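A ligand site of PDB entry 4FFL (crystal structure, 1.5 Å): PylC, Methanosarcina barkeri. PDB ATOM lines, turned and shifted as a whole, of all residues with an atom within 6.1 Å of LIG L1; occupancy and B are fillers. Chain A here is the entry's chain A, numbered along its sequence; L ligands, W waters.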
ATOM      1  N   VAL A   7       3.725  14.078   6.273  1.00  0.00           N
ATOM      2  CA  VAL A   7       3.398  13.641   7.637  1.00  0.00           C
ATOM      3  C   VAL A   7       4.415  14.270   8.586  1.00  0.00           C
ATOM      4  O   VAL A   7       5.528  13.761   8.748  1.00  0.00           O
ATOM      5  CB  VAL A   7       3.342  12.107   7.774  1.00  0.00           C
ATOM      6  CG1 VAL A   7       2.931  11.707   9.185  1.00  0.00           C
ATOM      7  CG2 VAL A   7       2.365  11.507   6.760  1.00  0.00           C
ATOM      8  N   GLY A   8       4.017  15.386   9.198  1.00  0.00           N
ATOM      9  CA  GLY A   8       4.901  16.170  10.061  1.00  0.00           C
ATOM     10  C   GLY A   8       4.977  17.611   9.576  1.00  0.00           C
ATOM     11  O   GLY A   8       5.362  17.875   8.436  1.00  0.00           O
ATOM     12  N   GLY A   9       4.621  18.537  10.457  1.00  0.00           N
ATOM     13  CA  GLY A   9       4.546  19.948  10.116  1.00  0.00           C
ATOM     14  C   GLY A   9       5.448  20.867  10.917  1.00  0.00           C
ATOM     15  O   GLY A   9       5.060  21.978  11.265  1.00  0.00           O
ATOM     16  N   LYS A  10       6.662  20.403  11.209  1.00  0.00           N
ATOM     17  CA  LYS A  10       7.661  21.235  11.877  1.00  0.00           C
ATOM     18  C   LYS A  10       8.771  21.626  10.900  1.00  0.00           C
ATOM     19  O   LYS A  10       8.480  22.109   9.811  1.00  0.00           O
ATOM     20  CB  LYS A  10       8.178  20.575  13.162  1.00  0.00           C
ATOM     21  CG  LYS A  10       7.210  20.695  14.333  1.00  0.00           C
ATOM     22  CD  LYS A  10       7.794  20.200  15.642  1.00  0.00           C
ATOM     23  CE  LYS A  10       8.400  21.337  16.453  1.00  0.00           C
ATOM     24  NZ  LYS A  10       8.612  20.929  17.871  1.00  0.00           N
ATOM     25  N   LEU A  11      10.041  21.423  11.275  1.00  0.00           N
ATOM     26  CA  LEU A  11      11.147  21.952  10.474  1.00  0.00           C
ATOM     27  C   LEU A  11      11.400  21.192   9.174  1.00  0.00           C
ATOM     28  O   LEU A  11      11.606  21.808   8.129  1.00  0.00           O
ATOM     29  CB  LEU A  11      12.420  22.087  11.319  1.00  0.00           C
ATOM     30  CG  LEU A  11      12.294  22.969  12.560  1.00  0.00           C
ATOM     31  CD1 LEU A  11      13.626  23.055  13.293  1.00  0.00           C
ATOM     32  CD2 LEU A  11      11.770  24.356  12.223  1.00  0.00           C
ATOM     33  N   GLN A  12      11.393  19.860   9.241  1.00  0.00           N
ATOM     34  CA  GLN A  12      11.476  19.050   8.021  1.00  0.00           C
ATOM     35  C   GLN A  12      10.276  19.337   7.126  1.00  0.00           C
ATOM     36  O   GLN A  12      10.411  19.443   5.907  1.00  0.00           O
ATOM     37  CB  GLN A  12      11.495  17.564   8.339  1.00  0.00           C
ATOM     38  CG  GLN A  12      12.706  17.051   9.097  1.00  0.00           C
ATOM     39  CD  GLN A  12      12.556  15.577   9.419  1.00  0.00           C
ATOM     40  OE1 GLN A  12      12.237  15.210  10.549  1.00  0.00           O
ATOM     41  NE2 GLN A  12      12.736  14.737   8.410  1.00  0.00           N
ATOM     42  N   VAL A  30      -0.410  16.553   7.148  1.00  0.00           N
ATOM     43  CA  VAL A  30      -0.990  15.776   8.241  1.00  0.00           C
ATOM     44  C   VAL A  30      -0.109  15.951   9.480  1.00  0.00           C
ATOM     45  O   VAL A  30       1.103  15.715   9.423  1.00  0.00           O
ATOM     46  CB  VAL A  30      -1.098  14.278   7.889  1.00  0.00           C
ATOM     47  CG1 VAL A  30      -1.553  13.477   9.104  1.00  0.00           C
ATOM     48  CG2 VAL A  30      -2.060  14.073   6.729  1.00  0.00           C
ATOM     49  N   ASP A  31      -0.714  16.366  10.584  1.00  0.00           N
ATOM     50  CA  ASP A  31       0.004  16.500  11.854  1.00  0.00           C
ATOM     51  C   ASP A  31      -0.982  16.331  13.005  1.00  0.00           C
ATOM     52  O   ASP A  31      -2.111  16.806  12.925  1.00  0.00           O
ATOM     53  CB  ASP A  31       0.706  17.866  11.934  1.00  0.00           C
ATOM     54  CG  ASP A  31       1.816  17.897  12.963  1.00  0.00           C
ATOM     55  OD1 ASP A  31       1.538  17.722  14.170  1.00  0.00           O
ATOM     56  OD2 ASP A  31       2.981  18.112  12.575  1.00  0.00           O
ATOM     57  N   LYS A  32      -0.539  15.666  14.062  1.00  0.00           N
ATOM     58  CA  LYS A  32      -1.371  15.395  15.232  1.00  0.00           C
ATOM     59  C   LYS A  32      -1.565  16.630  16.137  1.00  0.00           C
ATOM     60  O   LYS A  32      -2.417  16.632  17.026  1.00  0.00           O
ATOM     61  CB  LYS A  32      -0.766  14.240  16.049  1.00  0.00           C
ATOM     62  CG  LYS A  32       0.638  14.535  16.560  1.00  0.00           C
ATOM     63  CD  LYS A  32       1.251  13.364  17.302  1.00  0.00           C
ATOM     64  CE  LYS A  32       2.639  13.732  17.815  1.00  0.00           C
ATOM     65  NZ  LYS A  32       3.337  12.590  18.457  1.00  0.00           N
ATOM     66  N   ASN A  33      -0.771  17.668  15.902  1.00  0.00           N
ATOM     67  CA  ASN A  33      -0.809  18.894  16.707  1.00  0.00           C
ATOM     68  C   ASN A  33      -1.660  19.970  16.036  1.00  0.00           C
ATOM     69  O   ASN A  33      -1.318  20.415  14.939  1.00  0.00           O
ATOM     70  CB  ASN A  33       0.629  19.412  16.937  1.00  0.00           C
ATOM     71  CG  ASN A  33       0.699  20.595  17.887  1.00  0.00           C
ATOM     72  OD1 ASN A  33      -0.303  21.034  18.470  1.00  0.00           O
ATOM     73  ND2 ASN A  33       1.906  21.137  18.059  1.00  0.00           N
ATOM     74  N   ALA A  36       0.376  22.785  14.942  1.00  0.00           N
ATOM     75  CA  ALA A  36       1.527  22.407  14.095  1.00  0.00           C
ATOM     76  C   ALA A  36       2.136  23.641  13.436  1.00  0.00           C
ATOM     77  O   ALA A  36       1.420  24.472  12.880  1.00  0.00           O
ATOM     78  CB  ALA A  36       1.115  21.388  13.054  1.00  0.00           C
ATOM     79  N   LEU A  37       3.452  23.726  13.505  1.00  0.00           N
ATOM     80  CA  LEU A  37       4.188  24.915  13.073  1.00  0.00           C
ATOM     81  C   LEU A  37       3.795  25.475  11.694  1.00  0.00           C
ATOM     82  O   LEU A  37       3.579  26.681  11.563  1.00  0.00           O
ATOM     83  CB  LEU A  37       5.696  24.646  13.144  1.00  0.00           C
ATOM     84  CG  LEU A  37       6.665  25.813  13.053  1.00  0.00           C
ATOM     85  CD1 LEU A  37       6.452  26.825  14.169  1.00  0.00           C
ATOM     86  CD2 LEU A  37       8.094  25.283  13.069  1.00  0.00           C
ATOM     87  N   PHE A  48      -4.747  14.922  12.572  1.00  0.00           N
ATOM     88  CA  PHE A  48      -4.975  13.629  13.198  1.00  0.00           C
ATOM     89  C   PHE A  48      -3.647  12.920  13.436  1.00  0.00           C
ATOM     90  O   PHE A  48      -2.618  13.299  12.861  1.00  0.00           O
ATOM     91  CB  PHE A  48      -5.952  12.744  12.387  1.00  0.00           C
ATOM     92  CG  PHE A  48      -5.434  12.314  11.040  1.00  0.00           C
ATOM     93  CD1 PHE A  48      -5.595  13.127   9.912  1.00  0.00           C
ATOM     94  CD2 PHE A  48      -4.824  11.072  10.885  1.00  0.00           C
ATOM     95  CE1 PHE A  48      -5.137  12.721   8.675  1.00  0.00           C
ATOM     96  CE2 PHE A  48      -4.356  10.659   9.636  1.00  0.00           C
ATOM     97  CZ  PHE A  48      -4.514  11.489   8.535  1.00  0.00           C
ATOM     98  N   ASP A  49      -3.664  11.913  14.309  1.00  0.00           N
ATOM     99  CA  ASP A  49      -2.496  11.095  14.578  1.00  0.00           C
ATOM    100  C   ASP A  49      -2.564   9.870  13.663  1.00  0.00           C
ATOM    101  O   ASP A  49      -3.529   9.096  13.733  1.00  0.00           O
ATOM    102  CB  ASP A  49      -2.470  10.672  16.059  1.00  0.00           C
ATOM    103  CG  ASP A  49      -1.174   9.988  16.463  1.00  0.00           C
ATOM    104  OD1 ASP A  49      -0.706   9.105  15.730  1.00  0.00           O
ATOM    105  OD2 ASP A  49      -0.616  10.341  17.535  1.00  0.00           O
ATOM    106  N   VAL A  50      -1.556   9.698  12.814  1.00  0.00           N
ATOM    107  CA  VAL A  50      -1.593   8.624  11.807  1.00  0.00           C
ATOM    108  C   VAL A  50      -1.586   7.217  12.420  1.00  0.00           C
ATOM    109  O   VAL A  50      -2.087   6.279  11.797  1.00  0.00           O
ATOM    110  CB  VAL A  50      -0.482   8.751  10.730  1.00  0.00           C
ATOM    111  CG1 VAL A  50      -0.561  10.088  10.019  1.00  0.00           C
ATOM    112  CG2 VAL A  50       0.904   8.545  11.333  1.00  0.00           C
ATOM    113  N   ILE A  51      -1.048   7.084  13.624  1.00  0.00           N
ATOM    114  CA  ILE A  51      -1.039   5.812  14.346  1.00  0.00           C
ATOM    115  C   ILE A  51      -2.432   5.481  14.875  1.00  0.00           C
ATOM    116  O   ILE A  51      -2.846   4.323  14.879  1.00  0.00           O
ATOM    117  CB  ILE A  51      -0.013   5.809  15.521  1.00  0.00           C
ATOM    118  CG1 ILE A  51       1.381   6.241  15.035  1.00  0.00           C
ATOM    119  CG2 ILE A  51       0.049   4.444  16.192  1.00  0.00           C
ATOM    120  CD1 ILE A  51       2.359   6.499  16.162  1.00  0.00           C
ATOM    121  N   VAL A  70       7.904  13.351   7.247  1.00  0.00           N
ATOM    122  CA  VAL A  70       8.834  14.424   7.627  1.00  0.00           C
ATOM    123  C   VAL A  70       8.746  14.636   9.131  1.00  0.00           C
ATOM    124  O   VAL A  70       8.395  15.717   9.620  1.00  0.00           O
ATOM    125  CB  VAL A  70       8.628  15.728   6.824  1.00  0.00           C
ATOM    126  CG1 VAL A  70       9.536  15.754   5.601  1.00  0.00           C
ATOM    127  CG2 VAL A  70       7.165  15.910   6.416  1.00  0.00           C
ATOM    128  N   ASN A  71       9.063  13.572   9.854  1.00  0.00           N
ATOM    129  CA  ASN A  71       9.185  13.612  11.306  1.00  0.00           C
ATOM    130  C   ASN A  71      10.166  12.544  11.769  1.00  0.00           C
ATOM    131  O   ASN A  71      10.500  11.632  11.011  1.00  0.00           O
ATOM    132  CB  ASN A  71       7.819  13.449  11.980  1.00  0.00           C
ATOM    133  CG  ASN A  71       7.270  12.033  11.869  1.00  0.00           C
ATOM    134  OD1 ASN A  71       7.633  11.148  12.639  1.00  0.00           O
ATOM    135  ND2 ASN A  71       6.353  11.827  10.926  1.00  0.00           N
ATOM    136  N   GLU A  72      10.630  12.680  13.007  1.00  0.00           N
ATOM    137  CA  GLU A  72      11.568  11.718  13.581  1.00  0.00           C
ATOM    138  C   GLU A  72      10.980  11.039  14.820  1.00  0.00           C
ATOM    139  O   GLU A  72      11.705  10.668  15.749  1.00  0.00           O
ATOM    140  CB  GLU A  72      12.900  12.406  13.897  1.00  0.00           C
ATOM    141  CG  GLU A  72      13.619  12.932  12.668  1.00  0.00           C
ATOM    142  CD  GLU A  72      14.816  13.777  13.018  1.00  0.00           C
ATOM    143  OE1 GLU A  72      14.634  14.869  13.583  1.00  0.00           O
ATOM    144  OE2 GLU A  72      15.949  13.340  12.723  1.00  0.00           O
ATOM    145  N   ASN A  73       9.656  10.875  14.823  1.00  0.00           N
ATOM    146  CA  ASN A  73       8.976  10.110  15.856  1.00  0.00           C
ATOM    147  C   ASN A  73       9.077   8.636  15.496  1.00  0.00           C
ATOM    148  O   ASN A  73       8.441   8.178  14.549  1.00  0.00           O
ATOM    149  CB  ASN A  73       7.495  10.561  15.947  1.00  0.00           C
ATOM    150  CG  ASN A  73       6.658   9.694  16.875  1.00  0.00           C
ATOM    151  OD1 ASN A  73       7.181   8.832  17.588  1.00  0.00           O
ATOM    152  ND2 ASN A  73       5.352   9.910  16.869  1.00  0.00           N
ATOM    153  N   ALA A  75       7.923   5.946  16.813  1.00  0.00           N
ATOM    154  CA  ALA A  75       6.626   5.267  16.857  1.00  0.00           C
ATOM    155  C   ALA A  75       5.878   5.464  15.532  1.00  0.00           C
ATOM    156  O   ALA A  75       5.312   4.520  14.997  1.00  0.00           O
ATOM    157  CB  ALA A  75       5.806   5.779  18.018  1.00  0.00           C
ATOM    158  N   CYS A  76       5.893   6.696  15.013  1.00  0.00           N
ATOM    159  CA  CYS A  76       5.261   6.997  13.738  1.00  0.00           C
ATOM    160  C   CYS A  76       5.952   6.272  12.577  1.00  0.00           C
ATOM    161  O   CYS A  76       5.286   5.644  11.750  1.00  0.00           O
ATOM    162  CB  CYS A  76       5.257   8.513  13.484  1.00  0.00           C
ATOM    163  SG  CYS A  76       4.448   9.000  11.940  1.00  0.00           S
ATOM    164  N   SER A 306      11.959  25.560  16.685  1.00  0.00           N
ATOM    165  CA  SER A 306      11.086  24.446  17.080  1.00  0.00           C
ATOM    166  C   SER A 306      10.092  24.803  18.192  1.00  0.00           C
ATOM    167  O   SER A 306       9.132  24.055  18.428  1.00  0.00           O
ATOM    168  CB  SER A 306      11.935  23.240  17.498  1.00  0.00           C
ATOM    169  OG  SER A 306      12.552  23.451  18.751  1.00  0.00           O
HETATM  170  P1  LIG L   1       7.216  17.578  19.052  1.00  0.00           P
HETATM  171  O1  LIG L   1       8.249  17.605  20.149  1.00  0.00           O
HETATM  172  O2  LIG L   1       6.519  18.893  18.814  1.00  0.00           O
HETATM  173  O3  LIG L   1       6.274  16.389  19.120  1.00  0.00           O
HETATM  174  P2  LIG L   1       9.650  17.290  17.558  1.00  0.00           P
HETATM  175  O4  LIG L   1      10.190  18.698  17.565  1.00  0.00           O
HETATM  176  O5  LIG L   1      10.244  16.289  18.504  1.00  0.00           O
HETATM  177  O6  LIG L   1       8.035  17.326  17.685  1.00  0.00           O
HETATM  178  P3  LIG L   1       9.239  15.359  15.467  1.00  0.00           P
HETATM  179  O7  LIG L   1       9.038  14.334  16.556  1.00  0.00           O
HETATM  180  O8  LIG L   1      10.107  15.006  14.282  1.00  0.00           O
HETATM  181  O9  LIG L   1       9.794  16.755  16.044  1.00  0.00           O
HETATM  182  O10 LIG L   1       7.779  15.726  14.899  1.00  0.00           O
HETATM  183  C1  LIG L   1       7.622  16.643  13.824  1.00  0.00           C
HETATM  184  C2  LIG L   1       6.135  16.831  13.576  1.00  0.00           C
HETATM  185  O11 LIG L   1       5.547  15.573  13.216  1.00  0.00           O
HETATM  186  C3  LIG L   1       5.424  17.339  14.825  1.00  0.00           C
HETATM  187  O12 LIG L   1       4.670  18.512  14.510  1.00  0.00           O
HETATM  188  C4  LIG L   1       4.525  16.174  15.234  1.00  0.00           C
HETATM  189  O13 LIG L   1       3.306  16.598  15.846  1.00  0.00           O
HETATM  190  C5  LIG L   1       4.326  15.422  13.918  1.00  0.00           C
HETATM  191  N1  LIG L   1       4.039  13.999  14.200  1.00  0.00           N
HETATM  192  C6  LIG L   1       4.823  13.132  14.878  1.00  0.00           C
HETATM  193  N2  LIG L   1       4.235  11.921  14.975  1.00  0.00           N
HETATM  194  C7  LIG L   1       3.049  12.002  14.351  1.00  0.00           C
HETATM  195  C8  LIG L   1       1.915  11.076  14.084  1.00  0.00           C
HETATM  196  N3  LIG L   1       1.959   9.801  14.522  1.00  0.00           N
HETATM  197  N4  LIG L   1       0.859  11.565  13.384  1.00  0.00           N
HETATM  198  C9  LIG L   1       0.817  12.843  12.956  1.00  0.00           C
HETATM  199  N5  LIG L   1       1.800  13.735  13.159  1.00  0.00           N
HETATM  200  C10 LIG L   1       2.912  13.376  13.843  1.00  0.00           C
HETATM  201  N1  LG2 L   2      12.197  16.288  13.148  1.00  0.00           N
HETATM  202  C1  LG2 L   2      12.318  17.665  13.690  1.00  0.00           C
HETATM  203  C2  LG2 L   2      11.444  18.630  12.920  1.00  0.00           C
HETATM  204  O1  LG2 L   2      11.247  19.762  13.323  1.00  0.00           O
HETATM  205  C3  LG2 L   2      13.811  18.094  13.701  1.00  0.00           C
HETATM  206  C4  LG2 L   2      14.449  18.186  12.288  1.00  0.00           C
HETATM  207  C5  LG2 L   2      15.897  18.740  12.381  1.00  0.00           C
HETATM  208  C6  LG2 L   2      16.659  18.551  11.045  1.00  0.00           C
HETATM  209  N2  LG2 L   2      17.855  19.418  11.015  1.00  0.00           N
HETATM  210  O2  LG2 L   2      10.944  18.172  11.766  1.00  0.00           O
HETATM  211  O   HOH W   1       2.831  17.281  18.830  1.00  0.00           O
HETATM  212  O   HOH W   2      12.430  13.706  17.928  1.00  0.00           O
HETATM  213  O   HOH W   3      11.867  20.351  15.900  1.00  0.00           O
HETATM  214  O   HOH W   4       9.780  13.849  18.900  1.00  0.00           O
HETATM  215  O   HOH W   5      13.007  16.232  16.624  1.00  0.00           O
HETATM  216  O   HOH W   6       6.334  13.688  17.694  1.00  0.00           O
HETATM  217  O   HOH W   7       4.225  19.864  16.990  1.00  0.00           O
HETATM  218  O   HOH W   8       2.214  10.138  17.689  1.00  0.00           O
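OD2 of Asp 31 sits at hydrogen-bond distance from O12 of LIG L1 (2.6 Å). O8 of LIG L1 is in hydrogen-bond range of N of Glu 72. NZ of Lys 10 is in salt-bridge range of O4 of LIG L1 (2.7 Å). N2 of LIG L1 is in hydrogen-bond range of ND2 of Asn 73 (3.0 Å). The side-chain carboxylate (OD1) of Asp 49 is in hydrogen-bond range of a nitrogen (N3) of LIG L1 (3.0 Å). N of Val 50 lies within hydrogen-bond range of N4 of LIG L1 (3.1 Å). The backbone NH of Lys 32 sits at hydrogen-bond distance from a nitrogen (N5) of LIG L1 (3.2 Å). N3 of LIG L1 sits at hydrogen-bond distance from SG of Cys 76 (3.7 Å). N1 of LG2 L2 lies within salt-bridge range of OE1 of Glu 72 (2.9 Å). O2 of LG2 L2 is in hydrogen-bond range of N of Gln 12. OE1 of Gln 12 is in hydrogen-bond range of N1 of LG2 L2 (2.8 Å). An oxygen (O1) of LG2 L2 lies within hydrogen-bond range of the backbone NH (N) of Leu 11 (2.9 Å).
An oxygen (O8) of LIG L1 lies within hydrogen-bond range of a nitrogen (N1) of LG2 L2 (2.7 Å).
O of Asp 31 sits at hydrogen-bond distance from N of Phe 48, 3.3 Å away. The side-chain carboxylate of Asp 31 sits at hydrogen-bond distance from the backbone NH of Gly 9. N of Asn 33 sits at hydrogen-bond distance from OD1 of Asp 31, at 2.9 Å. The side-chain amino group (NZ) of Lys 10 sits at hydrogen-bond distance from the backbone carbonyl oxygen (O) of Ser 306. N of Asn 73 lies within hydrogen-bond range of OD1 of Asn 71 (3.0 Å). N of Lys 32 sits at hydrogen-bond distance from O of Phe 48, 3.4 Å away. The backbone NH of Gly 8 sits at hydrogen-bond distance from the backbone carbonyl oxygen of Val 30, 2.9 Å away. N of Leu 37 sits at hydrogen-bond distance from O of Gly 9 (3.3 Å).
Gly 8 touches LIG L1. Gly 9 touches LIG L1. Phe 48 touches LIG L1 (O to C9, 3.5 Å). CG1 of Ile 51 touches N3 of LIG L1, 3.6 Å away. CB of Asn 71 touches O11 of LIG L1 (3.3 Å). Hydrophobic or aromatic side chains that line LIG L1: Val 50 and Ile 51. Within 4 Å of LIG L1: Gly 8, Gly 9, Lys 10, Asp 31, Lys 32, Phe 48, Asp 49, Val 50, Ile 51, Asn 71, Glu 72, Asn 73 and Cys 76.
Water W7 bridges the side-chain amide nitrogen of Asn 33 (2.9 Å) and an oxygen (O12) of LIG L1 (2.9 Å). Water W3 bridges O1 of LG2 L2 and O4 of LIG L1. Water W6 bridges O7 of LIG L1 (3.0 Å) and NZ of Lys 32 (3.3 Å).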
